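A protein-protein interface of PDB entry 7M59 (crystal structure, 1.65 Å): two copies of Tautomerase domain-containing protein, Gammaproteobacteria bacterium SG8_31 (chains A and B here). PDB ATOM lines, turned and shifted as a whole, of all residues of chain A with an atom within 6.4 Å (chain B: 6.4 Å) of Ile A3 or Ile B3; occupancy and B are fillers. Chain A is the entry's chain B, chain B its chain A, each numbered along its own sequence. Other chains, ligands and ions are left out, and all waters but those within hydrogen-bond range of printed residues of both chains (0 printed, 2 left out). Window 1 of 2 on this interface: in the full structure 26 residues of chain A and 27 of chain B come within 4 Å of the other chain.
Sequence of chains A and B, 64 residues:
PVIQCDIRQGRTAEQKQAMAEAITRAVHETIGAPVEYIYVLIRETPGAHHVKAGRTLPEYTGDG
Among the printed residues, merely in contact across the chains: Pro A1 with Asp B6 (3.2 Å), Pro A1 with Ile B7 (3.99 Å), Val A2 with Gln B4 (3.5 Å), Val A2 with Cys B5 (3.6 Å), Ile A3 with Ile B3 (3.6 Å), Ile A3 with Gln B4 (3.2 Å), Ile A3 with Cys B5 (3.8 Å), Gln A4 with Ile B3 (3.2 Å), Gln A4 with Asp B6 (3.96 Å), Cys A5 with Val B2 (3.6 Å), Cys A5 with Ile B3 (3.9 Å), Asp A6 with Pro B1 (3.3 Å), Asp A6 with Gln B4 (3.9 Å), Ile A7 with Pro B1 (3.97 Å), Ile A23 with Val B27 (3.97 Å) and Val A27 with Ile B23 (3.96 Å).
Pro A1 touches Ile B7, and with the chains exchanged Ile A7 touches Pro B1. Ile B3 touches its own counterpart, Ile A3. Ile A3 touches Gln B4, and with the chains exchanged Gln A4 touches Ile B3. Gln A4 touches Asp B6, and with the chains exchanged Asp A6 touches Gln B4. Positions printed for both chains: 1, 2, 3, 4, 5, 6, 7, 19, 23, 27, 38, 39, 40, 41 and 42. Of the 20 pairs that touch across the chains among the printed residues, 20 have their exchanged pair printed and touching as well.
The backbone carbonyl oxygen (O) of Ile B3 lies within hydrogen-bond range of the backbone NH (N) of Leu B41, 2.9 Å away. The backbone carbonyl oxygen of Tyr A39 sits at hydrogen-bond distance from the backbone NH of Ile A3 (2.8 Å). N of Tyr A39 is in hydrogen-bond range of O of Pro A1, at 3.0 Å. The backbone carbonyl oxygen of Ile A3 sits at hydrogen-bond distance from the backbone NH of Leu A41 (2.8 Å). N of Cys A5 lies within hydrogen-bond range of O of Leu A41 (2.8 Å). The backbone NH of Ile B3 lies within hydrogen-bond range of the backbone carbonyl oxygen of Tyr B39 (2.9 Å).
Ile A3 touches just these residues of chain B: Ile B3 (3.6 Å), Gln B4 (3.2 Å) and Cys B5 (3.8 Å). Of the printed residues of chain A, Val B2 touches Gln A4 (3.4 Å), Cys A5 (3.6 Å) and Asp A6 (2.9 Å). Of the printed residues of chain A, Ile B3 touches Ile A3, Gln A4 and Cys A5. Printed residues of chain A within 4 Å of Gln B4: Val A2, Ile A3, Gln A4 and Asp A6. Met B19 touches none of the printed residues of chain A. Printed residues of chain A within 4 Å of Ile B23: Val A27 (3.96 Å). Ile B38 touches none of the printed residues of chain A. The nearest printed residue of chain A that does not touch Asp B6 is Ile A3 (4.8 Å).
Printed residues of chain B that touch a printed residue of chain A: Pro B1, Val B2, Ile B3, Gln B4, Cys B5, Asp B6, Ile B7, Ile B23 and Val B27. Hydrophobic or aromatic side chains of chain B within 4 Å of the printed part of chain A: Pro B1, Ile B3, Ile B7, Ile B23 and Val B27. Among the printed residues, 20 pairs touch across the chains. Among the printed residues, no Asp or Glu carboxylate lies within 4 Å of a Lys or Arg side-chain nitrogen of the other chain.
The backbone carbonyl oxygen (O) of Gln B4 lies within hydrogen-bond range of the backbone NH (N) of Gln A4 (2.8 Å). The backbone carbonyl oxygen of Val B2 lies close to the backbone carbonyl oxygen of Gln A4 (3.4 Å). The backbone NH (N) of Asp B6 is in hydrogen-bond range of the backbone carbonyl oxygen (O) of Val A2 (2.9 Å). The backbone NH (N) of Asp A6 sits at hydrogen-bond distance from the backbone carbonyl oxygen (O) of Val B2, 2.9 Å away.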
ATOM      1  N   PRO A   1      26.774 -20.287  32.315  1.00  0.00           N
ATOM      2  CA  PRO A   1      27.083 -18.863  32.121  1.00  0.00           C
ATOM      3  C   PRO A   1      25.820 -18.034  32.113  1.00  0.00           C
ATOM      4  O   PRO A   1      24.734 -18.578  31.911  1.00  0.00           O
ATOM      5  CB  PRO A   1      27.745 -18.824  30.743  1.00  0.00           C
ATOM      6  CG  PRO A   1      27.155 -20.018  30.031  1.00  0.00           C
ATOM      7  CD  PRO A   1      27.093 -21.073  31.107  1.00  0.00           C
ATOM      8  N   VAL A   2      25.957 -16.725  32.316  1.00  0.00           N
ATOM      9  CA  VAL A   2      24.834 -15.797  32.229  1.00  0.00           C
ATOM     10  C   VAL A   2      25.006 -14.983  30.954  1.00  0.00           C
ATOM     11  O   VAL A   2      26.074 -14.401  30.728  1.00  0.00           O
ATOM     12  CB  VAL A   2      24.766 -14.873  33.461  1.00  0.00           C
ATOM     13  CG1 VAL A   2      23.594 -13.882  33.334  1.00  0.00           C
ATOM     14  CG2 VAL A   2      24.649 -15.682  34.746  1.00  0.00           C
ATOM     15  N   ILE A   3      23.969 -14.943  30.116  1.00  0.00           N
ATOM     16  CA  ILE A   3      23.993 -14.138  28.892  1.00  0.00           C
ATOM     17  C   ILE A   3      22.884 -13.097  29.006  1.00  0.00           C
ATOM     18  O   ILE A   3      21.700 -13.450  28.967  1.00  0.00           O
ATOM     19  CB  ILE A   3      23.807 -14.983  27.622  1.00  0.00           C
ATOM     20  CG1 ILE A   3      24.662 -16.268  27.652  1.00  0.00           C
ATOM     21  CG2 ILE A   3      24.094 -14.125  26.389  1.00  0.00           C
ATOM     22  CD1 ILE A   3      26.186 -16.032  27.615  1.00  0.00           C
ATOM     23  N   GLN A   4      23.253 -11.825  29.152  1.00  0.00           N
ATOM     24  CA  GLN A   4      22.280 -10.744  29.272  1.00  0.00           C
ATOM     25  C   GLN A   4      22.131 -10.055  27.929  1.00  0.00           C
ATOM     26  O   GLN A   4      23.130  -9.658  27.318  1.00  0.00           O
ATOM     27  CB  GLN A   4      22.699  -9.719  30.326  1.00  0.00           C
ATOM     28  CG  GLN A   4      22.693 -10.265  31.747  1.00  0.00           C
ATOM     29  CD  GLN A   4      23.328  -9.310  32.719  1.00  0.00           C
ATOM     30  OE1 GLN A   4      22.660  -8.407  33.249  1.00  0.00           O
ATOM     31  NE2 GLN A   4      24.632  -9.475  32.951  1.00  0.00           N
ATOM     32  N   CYS A   5      20.887  -9.899  27.481  1.00  0.00           N
ATOM     33  CA  CYS A   5      20.585  -9.346  26.162  1.00  0.00           C
ATOM     34  C   CYS A   5      19.741  -8.101  26.357  1.00  0.00           C
ATOM     35  O   CYS A   5      18.545  -8.211  26.634  1.00  0.00           O
ATOM     36  CB  CYS A   5      19.836 -10.353  25.304  1.00  0.00           C
ATOM     37  SG  CYS A   5      20.663 -11.937  25.197  1.00  0.00           S
ATOM     38  N   ASP A   6      20.346  -6.925  26.204  1.00  0.00           N
ATOM     39  CA  ASP A   6      19.620  -5.659  26.267  1.00  0.00           C
ATOM     40  C   ASP A   6      19.299  -5.263  24.833  1.00  0.00           C
ATOM     41  O   ASP A   6      20.179  -4.804  24.095  1.00  0.00           O
ATOM     42  CB  ASP A   6      20.448  -4.586  26.962  1.00  0.00           C
ATOM     43  CG  ASP A   6      20.476  -4.761  28.474  1.00  0.00           C
ATOM     44  OD1 ASP A   6      19.516  -4.307  29.135  1.00  0.00           O
ATOM     45  OD2 ASP A   6      21.475  -5.321  28.979  1.00  0.00           O
ATOM     46  N   ILE A   7      18.037  -5.448  24.446  1.00  0.00           N
ATOM     47  CA  ILE A   7      17.601  -5.253  23.071  1.00  0.00           C
ATOM     48  C   ILE A   7      16.525  -4.177  23.043  1.00  0.00           C
ATOM     49  O   ILE A   7      15.924  -3.823  24.063  1.00  0.00           O
ATOM     50  CB  ILE A   7      17.083  -6.568  22.444  1.00  0.00           C
ATOM     51  CG1 ILE A   7      15.743  -6.974  23.075  1.00  0.00           C
ATOM     52  CG2 ILE A   7      18.125  -7.674  22.619  1.00  0.00           C
ATOM     53  CD1 ILE A   7      15.077  -8.218  22.431  1.00  0.00           C
ATOM     54  N   MET A  19      15.700 -16.039  19.543  1.00  0.00           N
ATOM     55  CA  MET A  19      16.995 -15.487  19.923  1.00  0.00           C
ATOM     56  C   MET A  19      17.591 -16.239  21.108  1.00  0.00           C
ATOM     57  O   MET A  19      18.769 -16.613  21.087  1.00  0.00           O
ATOM     58  CB  MET A  19      16.868 -13.996  20.249  1.00  0.00           C
ATOM     59  CG  MET A  19      18.226 -13.351  20.581  1.00  0.00           C
ATOM     60  SD  MET A  19      18.110 -11.659  21.195  1.00  0.00           S
ATOM     61  CE  MET A  19      17.418 -11.934  22.818  1.00  0.00           C
ATOM     62  N   ILE A  23      21.037 -18.352  20.951  1.00  0.00           N
ATOM     63  CA  ILE A  23      22.173 -17.998  21.803  1.00  0.00           C
ATOM     64  C   ILE A  23      22.581 -19.181  22.672  1.00  0.00           C
ATOM     65  O   ILE A  23      23.776 -19.452  22.860  1.00  0.00           O
ATOM     66  CB  ILE A  23      21.830 -16.757  22.649  1.00  0.00           C
ATOM     67  CG1 ILE A  23      21.852 -15.510  21.779  1.00  0.00           C
ATOM     68  CG2 ILE A  23      22.816 -16.607  23.826  1.00  0.00           C
ATOM     69  CD1 ILE A  23      21.386 -14.255  22.522  1.00  0.00           C
ATOM     70  N   VAL A  27      26.310 -20.725  22.479  1.00  0.00           N
ATOM     71  CA  VAL A  27      27.204 -20.790  23.630  1.00  0.00           C
ATOM     72  C   VAL A  27      27.627 -22.230  23.896  1.00  0.00           C
ATOM     73  O   VAL A  27      28.816 -22.523  24.077  1.00  0.00           O
ATOM     74  CB  VAL A  27      26.520 -20.160  24.859  1.00  0.00           C
ATOM     75  CG1 VAL A  27      27.304 -20.460  26.134  1.00  0.00           C
ATOM     76  CG2 VAL A  27      26.378 -18.661  24.643  1.00  0.00           C
ATOM     77  N   ILE A  38      23.362 -22.732  31.292  1.00  0.00           N
ATOM     78  CA  ILE A  38      23.176 -21.512  30.508  1.00  0.00           C
ATOM     79  C   ILE A  38      21.904 -20.810  30.961  1.00  0.00           C
ATOM     80  O   ILE A  38      20.840 -21.433  31.080  1.00  0.00           O
ATOM     81  CB  ILE A  38      23.140 -21.826  29.002  1.00  0.00           C
ATOM     82  CG1 ILE A  38      24.471 -22.474  28.569  1.00  0.00           C
ATOM     83  CG2 ILE A  38      22.845 -20.558  28.198  1.00  0.00           C
ATOM     84  CD1 ILE A  38      24.514 -22.868  27.086  1.00  0.00           C
ATOM     85  N   TYR A  39      22.013 -19.509  31.228  1.00  0.00           N
ATOM     86  CA  TYR A  39      20.882 -18.693  31.664  1.00  0.00           C
ATOM     87  C   TYR A  39      20.893 -17.436  30.807  1.00  0.00           C
ATOM     88  O   TYR A  39      21.830 -16.635  30.901  1.00  0.00           O
ATOM     89  CB  TYR A  39      21.009 -18.359  33.154  1.00  0.00           C
ATOM     90  CG  TYR A  39      19.769 -17.856  33.876  1.00  0.00           C
ATOM     91  CD1 TYR A  39      18.933 -16.885  33.319  1.00  0.00           C
ATOM     92  CD2 TYR A  39      19.472 -18.313  35.152  1.00  0.00           C
ATOM     93  CE1 TYR A  39      17.819 -16.403  34.017  1.00  0.00           C
ATOM     94  CE2 TYR A  39      18.355 -17.843  35.848  1.00  0.00           C
ATOM     95  CZ  TYR A  39      17.538 -16.891  35.274  1.00  0.00           C
ATOM     96  OH  TYR A  39      16.447 -16.421  35.985  1.00  0.00           O
ATOM     97  N   VAL A  40      19.890 -17.296  29.937  1.00  0.00           N
ATOM     98  CA  VAL A  40      19.748 -16.131  29.069  1.00  0.00           C
ATOM     99  C   VAL A  40      18.701 -15.220  29.684  1.00  0.00           C
ATOM    100  O   VAL A  40      17.621 -15.675  30.082  1.00  0.00           O
ATOM    101  CB  VAL A  40      19.355 -16.534  27.636  1.00  0.00           C
ATOM    102  CG1 VAL A  40      19.160 -15.288  26.753  1.00  0.00           C
ATOM    103  CG2 VAL A  40      20.402 -17.459  27.036  1.00  0.00           C
ATOM    104  N   LEU A  41      19.022 -13.933  29.772  1.00  0.00           N
ATOM    105  CA  LEU A  41      18.116 -12.943  30.326  1.00  0.00           C
ATOM    106  C   LEU A  41      17.915 -11.853  29.285  1.00  0.00           C
ATOM    107  O   LEU A  41      18.893 -11.307  28.753  1.00  0.00           O
ATOM    108  CB  LEU A  41      18.691 -12.381  31.630  1.00  0.00           C
ATOM    109  CG  LEU A  41      17.869 -11.284  32.269  1.00  0.00           C
ATOM    110  CD1 LEU A  41      16.554 -11.864  32.779  1.00  0.00           C
ATOM    111  CD2 LEU A  41      18.703 -10.746  33.397  1.00  0.00           C
ATOM    112  N   ILE A  42      16.653 -11.559  28.972  1.00  0.00           N
ATOM    113  CA  ILE A  42      16.283 -10.569  27.963  1.00  0.00           C
ATOM    114  C   ILE A  42      15.690  -9.344  28.647  1.00  0.00           C
ATOM    115  O   ILE A  42      14.754  -9.462  29.450  1.00  0.00           O
ATOM    116  CB  ILE A  42      15.281 -11.159  26.954  1.00  0.00           C
ATOM    117  CG1 ILE A  42      15.899 -12.374  26.265  1.00  0.00           C
ATOM    118  CG2 ILE A  42      14.858 -10.122  25.937  1.00  0.00           C
ATOM    119  CD1 ILE A  42      14.930 -13.076  25.306  1.00  0.00           C
ATOM    120  N   PRO B   1      22.125  -3.746  20.040  1.00  0.00           N
ATOM    121  CA  PRO B   1      21.899  -4.363  21.359  1.00  0.00           C
ATOM    122  C   PRO B   1      23.211  -4.682  22.046  1.00  0.00           C
ATOM    123  O   PRO B   1      24.241  -4.781  21.378  1.00  0.00           O
ATOM    124  CB  PRO B   1      21.149  -5.657  21.027  1.00  0.00           C
ATOM    125  CG  PRO B   1      21.604  -5.982  19.620  1.00  0.00           C
ATOM    126  CD  PRO B   1      21.708  -4.642  18.943  1.00  0.00           C
ATOM    127  N   VAL B   2      23.179  -4.846  23.365  1.00  0.00           N
ATOM    128  CA  VAL B   2      24.351  -5.255  24.129  1.00  0.00           C
ATOM    129  C   VAL B   2      24.110  -6.675  24.616  1.00  0.00           C
ATOM    130  O   VAL B   2      23.060  -6.959  25.205  1.00  0.00           O
ATOM    131  CB  VAL B   2      24.615  -4.303  25.308  1.00  0.00           C
ATOM    132  CG1 VAL B   2      25.847  -4.765  26.112  1.00  0.00           C
ATOM    133  CG2 VAL B   2      24.810  -2.879  24.799  1.00  0.00           C
ATOM    134  N   ILE B   3      25.066  -7.567  24.352  1.00  0.00           N
ATOM    135  CA  ILE B   3      25.006  -8.957  24.804  1.00  0.00           C
ATOM    136  C   ILE B   3      26.192  -9.170  25.731  1.00  0.00           C
ATOM    137  O   ILE B   3      27.338  -9.199  25.271  1.00  0.00           O
ATOM    138  CB  ILE B   3      25.045  -9.968  23.644  1.00  0.00           C
ATOM    139  CG1 ILE B   3      24.157  -9.523  22.461  1.00  0.00           C
ATOM    140  CG2 ILE B   3      24.669 -11.371  24.158  1.00  0.00           C
ATOM    141  CD1 ILE B   3      22.658  -9.509  22.776  1.00  0.00           C
ATOM    142  N   GLN B   4      25.930  -9.285  27.032  1.00  0.00           N
ATOM    143  CA  GLN B   4      26.982  -9.529  28.011  1.00  0.00           C
ATOM    144  C   GLN B   4      27.042 -11.017  28.301  1.00  0.00           C
ATOM    145  O   GLN B   4      26.010 -11.643  28.554  1.00  0.00           O
ATOM    146  CB  GLN B   4      26.743  -8.760  29.309  1.00  0.00           C
ATOM    147  CG  GLN B   4      26.781  -7.254  29.129  1.00  0.00           C
ATOM    148  CD  GLN B   4      26.292  -6.543  30.367  1.00  0.00           C
ATOM    149  OE1 GLN B   4      27.048  -6.345  31.328  1.00  0.00           O
ATOM    150  NE2 GLN B   4      25.017  -6.165  30.364  1.00  0.00           N
ATOM    151  N   CYS B   5      28.247 -11.570  28.278  1.00  0.00           N
ATOM    152  CA  CYS B   5      28.462 -13.007  28.438  1.00  0.00           C
ATOM    153  C   CYS B   5      29.399 -13.210  29.616  1.00  0.00           C
ATOM    154  O   CYS B   5      30.603 -12.972  29.497  1.00  0.00           O
ATOM    155  CB  CYS B   5      29.059 -13.615  27.170  1.00  0.00           C
ATOM    156  SG  CYS B   5      28.153 -13.229  25.676  1.00  0.00           S
ATOM    157  N   ASP B   6      28.856 -13.625  30.760  1.00  0.00           N
ATOM    158  CA  ASP B   6      29.675 -13.952  31.926  1.00  0.00           C
ATOM    159  C   ASP B   6      29.922 -15.452  31.908  1.00  0.00           C
ATOM    160  O   ASP B   6      29.034 -16.248  32.248  1.00  0.00           O
ATOM    161  CB  ASP B   6      28.998 -13.515  33.218  1.00  0.00           C
ATOM    162  CG  ASP B   6      29.103 -12.024  33.452  1.00  0.00           C
ATOM    163  OD1 ASP B   6      30.157 -11.568  33.961  1.00  0.00           O
ATOM    164  OD2 ASP B   6      28.123 -11.328  33.141  1.00  0.00           O
ATOM    165  N   ILE B   7      31.138 -15.837  31.518  1.00  0.00           N
ATOM    166  CA  ILE B   7      31.496 -17.234  31.309  1.00  0.00           C
ATOM    167  C   ILE B   7      32.633 -17.611  32.250  1.00  0.00           C
ATOM    168  O   ILE B   7      33.336 -16.760  32.797  1.00  0.00           O
ATOM    169  CB  ILE B   7      31.884 -17.504  29.841  1.00  0.00           C
ATOM    170  CG1 ILE B   7      33.228 -16.840  29.510  1.00  0.00           C
ATOM    171  CG2 ILE B   7      30.785 -17.006  28.908  1.00  0.00           C
ATOM    172  CD1 ILE B   7      33.712 -17.133  28.069  1.00  0.00           C
ATOM    173  N   MET B  19      32.432 -17.853  19.894  1.00  0.00           N
ATOM    174  CA  MET B  19      31.193 -17.576  20.612  1.00  0.00           C
ATOM    175  C   MET B  19      30.655 -16.198  20.261  1.00  0.00           C
ATOM    176  O   MET B  19      29.455 -16.035  20.011  1.00  0.00           O
ATOM    177  CB  MET B  19      31.412 -17.687  22.121  1.00  0.00           C
ATOM    178  CG  MET B  19      30.123 -17.498  22.917  1.00  0.00           C
ATOM    179  SD  MET B  19      30.384 -17.348  24.692  1.00  0.00           S
ATOM    180  CE  MET B  19      31.189 -15.757  24.830  1.00  0.00           C
ATOM    181  N   ILE B  23      27.087 -15.592  18.441  1.00  0.00           N
ATOM    182  CA  ILE B  23      26.041 -14.792  19.079  1.00  0.00           C
ATOM    183  C   ILE B  23      25.648 -13.620  18.191  1.00  0.00           C
ATOM    184  O   ILE B  23      24.462 -13.286  18.073  1.00  0.00           O
ATOM    185  CB  ILE B  23      26.498 -14.326  20.474  1.00  0.00           C
ATOM    186  CG1 ILE B  23      26.485 -15.512  21.438  1.00  0.00           C
ATOM    187  CG2 ILE B  23      25.586 -13.207  20.986  1.00  0.00           C
ATOM    188  CD1 ILE B  23      27.115 -15.227  22.814  1.00  0.00           C
ATOM    189  N   VAL B  27      21.829 -13.160  17.014  1.00  0.00           N
ATOM    190  CA  VAL B  27      21.017 -11.984  17.313  1.00  0.00           C
ATOM    191  C   VAL B  27      20.549 -11.318  16.023  1.00  0.00           C
ATOM    192  O   VAL B  27      19.371 -10.976  15.874  1.00  0.00           O
ATOM    193  CB  VAL B  27      21.803 -11.015  18.215  1.00  0.00           C
ATOM    194  CG1 VAL B  27      21.074  -9.677  18.353  1.00  0.00           C
ATOM    195  CG2 VAL B  27      22.013 -11.667  19.574  1.00  0.00           C
ATOM    196  N   ILE B  38      25.314  -4.321  17.065  1.00  0.00           N
ATOM    197  CA  ILE B  38      25.514  -5.389  18.042  1.00  0.00           C
ATOM    198  C   ILE B  38      26.855  -5.195  18.742  1.00  0.00           C
ATOM    199  O   ILE B  38      27.881  -4.937  18.100  1.00  0.00           O
ATOM    200  CB  ILE B  38      25.431  -6.770  17.375  1.00  0.00           C
ATOM    201  CG1 ILE B  38      24.031  -6.990  16.792  1.00  0.00           C
ATOM    202  CG2 ILE B  38      25.775  -7.861  18.375  1.00  0.00           C
ATOM    203  CD1 ILE B  38      23.904  -8.252  15.965  1.00  0.00           C
ATOM    204  N   TYR B  39      26.850  -5.320  20.069  1.00  0.00           N
ATOM    205  CA  TYR B  39      28.062  -5.220  20.874  1.00  0.00           C
ATOM    206  C   TYR B  39      28.041  -6.402  21.835  1.00  0.00           C
ATOM    207  O   TYR B  39      27.149  -6.494  22.686  1.00  0.00           O
ATOM    208  CB  TYR B  39      28.103  -3.881  21.613  1.00  0.00           C
ATOM    209  CG  TYR B  39      29.428  -3.420  22.203  1.00  0.00           C
ATOM    210  CD1 TYR B  39      29.820  -2.092  22.084  1.00  0.00           C
ATOM    211  CD2 TYR B  39      30.248  -4.282  22.942  1.00  0.00           C
ATOM    212  CE1 TYR B  39      31.002  -1.634  22.649  1.00  0.00           C
ATOM    213  CE2 TYR B  39      31.441  -3.826  23.509  1.00  0.00           C
ATOM    214  CZ  TYR B  39      31.803  -2.500  23.357  1.00  0.00           C
ATOM    215  OH  TYR B  39      32.961  -2.020  23.919  1.00  0.00           O
ATOM    216  N   VAL B  40      28.979  -7.329  21.659  1.00  0.00           N
ATOM    217  CA  VAL B  40      29.132  -8.487  22.533  1.00  0.00           C
ATOM    218  C   VAL B  40      30.292  -8.220  23.478  1.00  0.00           C
ATOM    219  O   VAL B  40      31.372  -7.792  23.051  1.00  0.00           O
ATOM    220  CB  VAL B  40      29.366  -9.776  21.729  1.00  0.00           C
ATOM    221  CG1 VAL B  40      29.551 -10.954  22.670  1.00  0.00           C
ATOM    222  CG2 VAL B  40      28.200 -10.027  20.789  1.00  0.00           C
ATOM    223  N   LEU B  41      30.074  -8.469  24.762  1.00  0.00           N
ATOM    224  CA  LEU B  41      31.080  -8.232  25.785  1.00  0.00           C
ATOM    225  C   LEU B  41      31.257  -9.514  26.582  1.00  0.00           C
ATOM    226  O   LEU B  41      30.274 -10.077  27.067  1.00  0.00           O
ATOM    227  CB  LEU B  41      30.655  -7.077  26.699  1.00  0.00           C
ATOM    228  CG  LEU B  41      31.569  -6.855  27.898  1.00  0.00           C
ATOM    229  CD1 LEU B  41      32.910  -6.297  27.413  1.00  0.00           C
ATOM    230  CD2 LEU B  41      30.892  -5.895  28.843  1.00  0.00           C
ATOM    231  N   ILE B  42      32.501  -9.980  26.705  1.00  0.00           N
ATOM    232  CA  ILE B  42      32.811 -11.231  27.388  1.00  0.00           C
ATOM    233  C   ILE B  42      33.552 -10.916  28.680  1.00  0.00           C
ATOM    234  O   ILE B  42      34.521 -10.146  28.679  1.00  0.00           O
ATOM    235  CB  ILE B  42      33.662 -12.159  26.505  1.00  0.00           C
ATOM    236  CG1 ILE B  42      32.917 -12.498  25.210  1.00  0.00           C
ATOM    237  CG2 ILE B  42      34.027 -13.420  27.285  1.00  0.00           C
ATOM    238  CD1 ILE B  42      33.822 -13.125  24.140  1.00  0.00           C
